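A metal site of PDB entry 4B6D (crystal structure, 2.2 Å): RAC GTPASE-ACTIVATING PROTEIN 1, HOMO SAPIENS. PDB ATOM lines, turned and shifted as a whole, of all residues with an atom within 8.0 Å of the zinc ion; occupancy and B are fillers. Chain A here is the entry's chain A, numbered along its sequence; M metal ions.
The zinc ion is bound by ND1 of His 9 (2.0 Å), SG of Cys 41 (2.3 Å), SG of Cys 38 (2.3 Å) and SG of Cys 57 (2.3 Å).
Of the 21 residues printed, 4 come within 4 Å of the zinc ion. Along chain A the residues within 4 Å of the zinc ion span positions 9 to 57.
The backbone NH (N) of Val 43 sits close to the side-chain sulfur (SG) of Cys 41, at 3.5 Å. The backbone NH (N) of Cys 57 sits at hydrogen-bond distance from the backbone carbonyl oxygen (O) of Arg 7 (2.8 Å). The backbone carbonyl oxygen (O) of Pro 54 sits at hydrogen-bond distance from a ring nitrogen (NE2) of His 9 (3.0 Å). The backbone NH (N) of Asp 10 lies close to the side-chain sulfur (SG) of Cys 38, at 3.4 Å. The side-chain sulfur of Cys 38 lies close to the backbone NH of Asp 40, 3.5 Å away. N of Cys 38 sits at hydrogen-bond distance from O of Val 43 (3.0 Å).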
ATOM      1  N   ARG A   7     -31.099 -21.834  29.863  1.00  0.00           N
ATOM      2  CA  ARG A   7     -29.792 -22.300  29.442  1.00  0.00           C
ATOM      3  C   ARG A   7     -28.974 -21.161  28.875  1.00  0.00           C
ATOM      4  O   ARG A   7     -29.364 -20.525  27.894  1.00  0.00           O
ATOM      5  CB  ARG A   7     -29.907 -23.419  28.417  1.00  0.00           C
ATOM      6  CG  ARG A   7     -30.021 -24.808  29.010  1.00  0.00           C
ATOM      7  CD  ARG A   7     -30.127 -25.837  27.900  1.00  0.00           C
ATOM      8  NE  ARG A   7     -28.836 -26.061  27.273  1.00  0.00           N
ATOM      9  CZ  ARG A   7     -27.958 -26.983  27.655  1.00  0.00           C
ATOM     10  NH1 ARG A   7     -28.245 -27.799  28.663  1.00  0.00           N
ATOM     11  NH2 ARG A   7     -26.798 -27.099  27.020  1.00  0.00           N
ATOM     12  N   LEU A   8     -27.836 -20.903  29.508  1.00  0.00           N
ATOM     13  CA  LEU A   8     -26.928 -19.864  29.061  1.00  0.00           C
ATOM     14  C   LEU A   8     -25.860 -20.458  28.156  1.00  0.00           C
ATOM     15  O   LEU A   8     -25.647 -21.675  28.125  1.00  0.00           O
ATOM     16  CB  LEU A   8     -26.299 -19.180  30.259  1.00  0.00           C
ATOM     17  CG  LEU A   8     -27.289 -18.536  31.225  1.00  0.00           C
ATOM     18  CD1 LEU A   8     -26.568 -17.950  32.440  1.00  0.00           C
ATOM     19  CD2 LEU A   8     -28.105 -17.468  30.524  1.00  0.00           C
ATOM     20  N   HIS A   9     -25.175 -19.589  27.420  1.00  0.00           N
ATOM     21  CA  HIS A   9     -24.091 -20.013  26.552  1.00  0.00           C
ATOM     22  C   HIS A   9     -22.835 -20.305  27.357  1.00  0.00           C
ATOM     23  O   HIS A   9     -22.655 -19.786  28.458  1.00  0.00           O
ATOM     24  CB  HIS A   9     -23.795 -18.936  25.506  1.00  0.00           C
ATOM     25  CG  HIS A   9     -24.930 -18.681  24.566  1.00  0.00           C
ATOM     26  ND1 HIS A   9     -25.233 -19.532  23.520  1.00  0.00           N
ATOM     27  CD2 HIS A   9     -25.838 -17.673  24.509  1.00  0.00           C
ATOM     28  CE1 HIS A   9     -26.276 -19.059  22.862  1.00  0.00           C
ATOM     29  NE2 HIS A   9     -26.665 -17.941  23.444  1.00  0.00           N
ATOM     30  N   ASP A  10     -21.966 -21.136  26.787  1.00  0.00           N
ATOM     31  CA  ASP A  10     -20.682 -21.425  27.395  1.00  0.00           C
ATOM     32  C   ASP A  10     -19.608 -20.769  26.548  1.00  0.00           C
ATOM     33  O   ASP A  10     -18.986 -21.400  25.704  1.00  0.00           O
ATOM     34  CB  ASP A  10     -20.455 -22.943  27.480  1.00  0.00           C
ATOM     35  CG  ASP A  10     -19.315 -23.308  28.405  1.00  0.00           C
ATOM     36  OD1 ASP A  10     -18.853 -22.441  29.159  1.00  0.00           O
ATOM     37  OD2 ASP A  10     -18.896 -24.492  28.376  1.00  0.00           O
ATOM     38  N   PHE A  11     -19.399 -19.479  26.793  1.00  0.00           N
ATOM     39  CA  PHE A  11     -18.510 -18.676  25.969  1.00  0.00           C
ATOM     40  C   PHE A  11     -17.033 -18.958  26.220  1.00  0.00           C
ATOM     41  O   PHE A  11     -16.596 -19.056  27.371  1.00  0.00           O
ATOM     42  CB  PHE A  11     -18.789 -17.182  26.162  1.00  0.00           C
ATOM     43  CG  PHE A  11     -20.072 -16.713  25.543  1.00  0.00           C
ATOM     44  CD1 PHE A  11     -20.273 -16.809  24.171  1.00  0.00           C
ATOM     45  CD2 PHE A  11     -21.072 -16.157  26.320  1.00  0.00           C
ATOM     46  CE1 PHE A  11     -21.441 -16.379  23.592  1.00  0.00           C
ATOM     47  CE2 PHE A  11     -22.254 -15.716  25.738  1.00  0.00           C
ATOM     48  CZ  PHE A  11     -22.437 -15.822  24.379  1.00  0.00           C
ATOM     49  N   LYS A  37     -17.286 -17.124  21.511  1.00  0.00           N
ATOM     50  CA  LYS A  37     -17.885 -18.193  20.728  1.00  0.00           C
ATOM     51  C   LYS A  37     -18.362 -19.272  21.691  1.00  0.00           C
ATOM     52  O   LYS A  37     -17.652 -19.643  22.623  1.00  0.00           O
ATOM     53  CB  LYS A  37     -16.853 -18.736  19.740  1.00  0.00           C
ATOM     54  CG  LYS A  37     -17.301 -19.913  18.897  1.00  0.00           C
ATOM     55  CD  LYS A  37     -16.242 -20.235  17.860  1.00  0.00           C
ATOM     56  CE  LYS A  37     -16.724 -21.260  16.855  1.00  0.00           C
ATOM     57  NZ  LYS A  37     -17.121 -22.544  17.499  1.00  0.00           N
ATOM     58  N   CYS A  38     -19.581 -19.767  21.466  1.00  0.00           N
ATOM     59  CA  CYS A  38     -20.146 -20.746  22.375  1.00  0.00           C
ATOM     60  C   CYS A  38     -19.623 -22.145  22.048  1.00  0.00           C
ATOM     61  O   CYS A  38     -19.521 -22.519  20.886  1.00  0.00           O
ATOM     62  CB  CYS A  38     -21.685 -20.717  22.293  1.00  0.00           C
ATOM     63  SG  CYS A  38     -22.526 -21.803  23.466  1.00  0.00           S
ATOM     64  N   ARG A  39     -19.287 -22.903  23.092  1.00  0.00           N
ATOM     65  CA  ARG A  39     -18.777 -24.254  22.910  1.00  0.00           C
ATOM     66  C   ARG A  39     -19.864 -25.193  22.429  1.00  0.00           C
ATOM     67  O   ARG A  39     -19.592 -26.192  21.763  1.00  0.00           O
ATOM     68  CB  ARG A  39     -18.176 -24.781  24.220  1.00  0.00           C
ATOM     69  CG  ARG A  39     -16.904 -24.058  24.656  1.00  0.00           C
ATOM     70  CD  ARG A  39     -16.426 -24.548  26.011  1.00  0.00           C
ATOM     71  NE  ARG A  39     -15.850 -25.889  25.930  1.00  0.00           N
ATOM     72  CZ  ARG A  39     -14.565 -26.138  25.727  1.00  0.00           C
ATOM     73  NH1 ARG A  39     -13.704 -25.134  25.569  1.00  0.00           N
ATOM     74  NH2 ARG A  39     -14.128 -27.392  25.665  1.00  0.00           N
ATOM     75  N   ASP A  40     -21.110 -24.875  22.769  1.00  0.00           N
ATOM     76  CA  ASP A  40     -22.237 -25.779  22.527  1.00  0.00           C
ATOM     77  C   ASP A  40     -22.992 -25.453  21.243  1.00  0.00           C
ATOM     78  O   ASP A  40     -23.483 -26.352  20.561  1.00  0.00           O
ATOM     79  CB  ASP A  40     -23.192 -25.757  23.722  1.00  0.00           C
ATOM     80  CG  ASP A  40     -22.521 -26.163  25.017  1.00  0.00           C
ATOM     81  OD1 ASP A  40     -21.663 -27.061  24.988  1.00  0.00           O
ATOM     82  OD2 ASP A  40     -22.858 -25.581  26.070  1.00  0.00           O
ATOM     83  N   CYS A  41     -23.099 -24.171  20.908  1.00  0.00           N
ATOM     84  CA  CYS A  41     -23.829 -23.756  19.714  1.00  0.00           C
ATOM     85  C   CYS A  41     -23.008 -22.883  18.767  1.00  0.00           C
ATOM     86  O   CYS A  41     -21.809 -22.708  18.945  1.00  0.00           O
ATOM     87  CB  CYS A  41     -25.133 -23.049  20.088  1.00  0.00           C
ATOM     88  SG  CYS A  41     -24.937 -21.415  20.820  1.00  0.00           S
ATOM     89  N   ARG A  42     -23.680 -22.350  17.746  1.00  0.00           N
ATOM     90  CA  ARG A  42     -23.023 -21.627  16.661  1.00  0.00           C
ATOM     91  C   ARG A  42     -22.854 -20.149  16.986  1.00  0.00           C
ATOM     92  O   ARG A  42     -22.285 -19.401  16.199  1.00  0.00           O
ATOM     93  CB  ARG A  42     -23.864 -21.764  15.388  1.00  0.00           C
ATOM     94  CG  ARG A  42     -24.011 -23.170  14.858  1.00  0.00           C
ATOM     95  CD  ARG A  42     -23.660 -23.287  13.389  1.00  0.00           C
ATOM     96  NE  ARG A  42     -23.999 -24.605  12.885  1.00  0.00           N
ATOM     97  CZ  ARG A  42     -23.161 -25.644  12.878  1.00  0.00           C
ATOM     98  NH1 ARG A  42     -21.928 -25.502  13.344  1.00  0.00           N
ATOM     99  NH2 ARG A  42     -23.555 -26.814  12.404  1.00  0.00           N
ATOM    100  N   VAL A  43     -23.355 -19.740  18.150  1.00  0.00           N
ATOM    101  CA  VAL A  43     -23.348 -18.324  18.529  1.00  0.00           C
ATOM    102  C   VAL A  43     -21.945 -17.726  18.699  1.00  0.00           C
ATOM    103  O   VAL A  43     -21.122 -18.234  19.455  1.00  0.00           O
ATOM    104  CB  VAL A  43     -24.182 -18.072  19.807  1.00  0.00           C
ATOM    105  CG1 VAL A  43     -23.868 -16.704  20.393  1.00  0.00           C
ATOM    106  CG2 VAL A  43     -25.660 -18.199  19.497  1.00  0.00           C
ATOM    107  N   VAL A  44     -21.697 -16.653  17.964  1.00  0.00           N
ATOM    108  CA  VAL A  44     -20.468 -15.887  18.093  1.00  0.00           C
ATOM    109  C   VAL A  44     -20.844 -14.404  18.214  1.00  0.00           C
ATOM    110  O   VAL A  44     -21.817 -13.970  17.597  1.00  0.00           O
ATOM    111  CB  VAL A  44     -19.524 -16.109  16.893  1.00  0.00           C
ATOM    112  CG1 VAL A  44     -20.222 -15.763  15.589  1.00  0.00           C
ATOM    113  CG2 VAL A  44     -18.237 -15.313  17.047  1.00  0.00           C
ATOM    114  N   CYS A  53     -27.114 -11.926  23.374  1.00  0.00           N
ATOM    115  CA  CYS A  53     -27.161 -13.147  22.574  1.00  0.00           C
ATOM    116  C   CYS A  53     -28.446 -13.909  22.863  1.00  0.00           C
ATOM    117  O   CYS A  53     -28.813 -14.098  24.020  1.00  0.00           O
ATOM    118  CB  CYS A  53     -25.953 -14.023  22.833  1.00  0.00           C
ATOM    119  SG  CYS A  53     -24.407 -13.383  22.161  1.00  0.00           S
ATOM    120  N   PRO A  54     -29.146 -14.346  21.796  1.00  0.00           N
ATOM    121  CA  PRO A  54     -30.416 -15.075  21.883  1.00  0.00           C
ATOM    122  C   PRO A  54     -30.371 -16.217  22.902  1.00  0.00           C
ATOM    123  O   PRO A  54     -29.456 -17.034  22.877  1.00  0.00           O
ATOM    124  CB  PRO A  54     -30.589 -15.651  20.482  1.00  0.00           C
ATOM    125  CG  PRO A  54     -29.657 -14.876  19.589  1.00  0.00           C
ATOM    126  CD  PRO A  54     -28.849 -13.935  20.416  1.00  0.00           C
ATOM    127  N   LEU A  55     -31.372 -16.252  23.780  1.00  0.00           N
ATOM    128  CA  LEU A  55     -31.495 -17.297  24.788  1.00  0.00           C
ATOM    129  C   LEU A  55     -32.790 -18.072  24.558  1.00  0.00           C
ATOM    130  O   LEU A  55     -33.745 -17.519  24.000  1.00  0.00           O
ATOM    131  CB  LEU A  55     -31.475 -16.693  26.182  1.00  0.00           C
ATOM    132  CG  LEU A  55     -30.116 -16.210  26.706  1.00  0.00           C
ATOM    133  CD1 LEU A  55     -30.256 -15.649  28.118  1.00  0.00           C
ATOM    134  CD2 LEU A  55     -29.107 -17.336  26.674  1.00  0.00           C
ATOM    135  N   PRO A  56     -32.841 -19.338  24.979  1.00  0.00           N
ATOM    136  CA  PRO A  56     -31.788 -20.112  25.666  1.00  0.00           C
ATOM    137  C   PRO A  56     -30.790 -20.726  24.695  1.00  0.00           C
ATOM    138  O   PRO A  56     -31.040 -20.745  23.487  1.00  0.00           O
ATOM    139  CB  PRO A  56     -32.588 -21.222  26.349  1.00  0.00           C
ATOM    140  CG  PRO A  56     -33.711 -21.456  25.412  1.00  0.00           C
ATOM    141  CD  PRO A  56     -34.083 -20.115  24.846  1.00  0.00           C
ATOM    142  N   CYS A  57     -29.676 -21.226  25.212  1.00  0.00           N
ATOM    143  CA  CYS A  57     -28.702 -21.933  24.403  1.00  0.00           C
ATOM    144  C   CYS A  57     -29.186 -23.336  24.046  1.00  0.00           C
ATOM    145  O   CYS A  57     -29.447 -24.160  24.914  1.00  0.00           O
ATOM    146  CB  CYS A  57     -27.353 -22.023  25.136  1.00  0.00           C
ATOM    147  SG  CYS A  57     -26.082 -22.974  24.277  1.00  0.00           S
ATOM    148  N   ILE A  58     -29.302 -23.601  22.741  1.00  0.00           N
ATOM    149  CA  ILE A  58     -29.673 -24.901  22.220  1.00  0.00           C
ATOM    150  C   ILE A  58     -28.465 -25.494  21.488  1.00  0.00           C
ATOM    151  O   ILE A  58     -28.145 -25.066  20.381  1.00  0.00           O
ATOM    152  CB  ILE A  58     -30.865 -24.816  21.253  1.00  0.00           C
ATOM    153  CG1 ILE A  58     -31.996 -23.979  21.864  1.00  0.00           C
ATOM    154  CG2 ILE A  58     -31.372 -26.209  20.897  1.00  0.00           C
ATOM    155  CD1 ILE A  58     -32.627 -24.593  23.084  1.00  0.00           C
ATOM    156  N   PRO A  59     -27.779 -26.463  22.123  1.00  0.00           N
ATOM    157  CA  PRO A  59     -26.555 -27.038  21.566  1.00  0.00           C
ATOM    158  C   PRO A  59     -26.729 -27.554  20.143  1.00  0.00           C
ATOM    159  O   PRO A  59     -27.757 -28.164  19.824  1.00  0.00           O
ATOM    160  CB  PRO A  59     -26.235 -28.206  22.502  1.00  0.00           C
ATOM    161  CG  PRO A  59     -27.234 -28.193  23.595  1.00  0.00           C
ATOM    162  CD  PRO A  59     -28.125 -27.004  23.450  1.00  0.00           C
ATOM    163  N   THR A  60     -25.739 -27.309  19.295  1.00  0.00           N
ATOM    164  CA  THR A  60     -25.784 -27.743  17.904  1.00  0.00           C
ATOM    165  C   THR A  60     -24.796 -28.876  17.666  1.00  0.00           C
ATOM    166  O   THR A  60     -25.083 -29.801  16.896  1.00  0.00           O
ATOM    167  CB  THR A  60     -25.469 -26.586  16.939  1.00  0.00           C
ATOM    168  OG1 THR A  60     -24.095 -26.189  17.090  1.00  0.00           O
ATOM    169  CG2 THR A  60     -26.367 -25.392  17.219  1.00  0.00           C
HETATM  170 ZN    ZN M   1     -24.770 -21.470  23.064  1.00  0.00          ZN
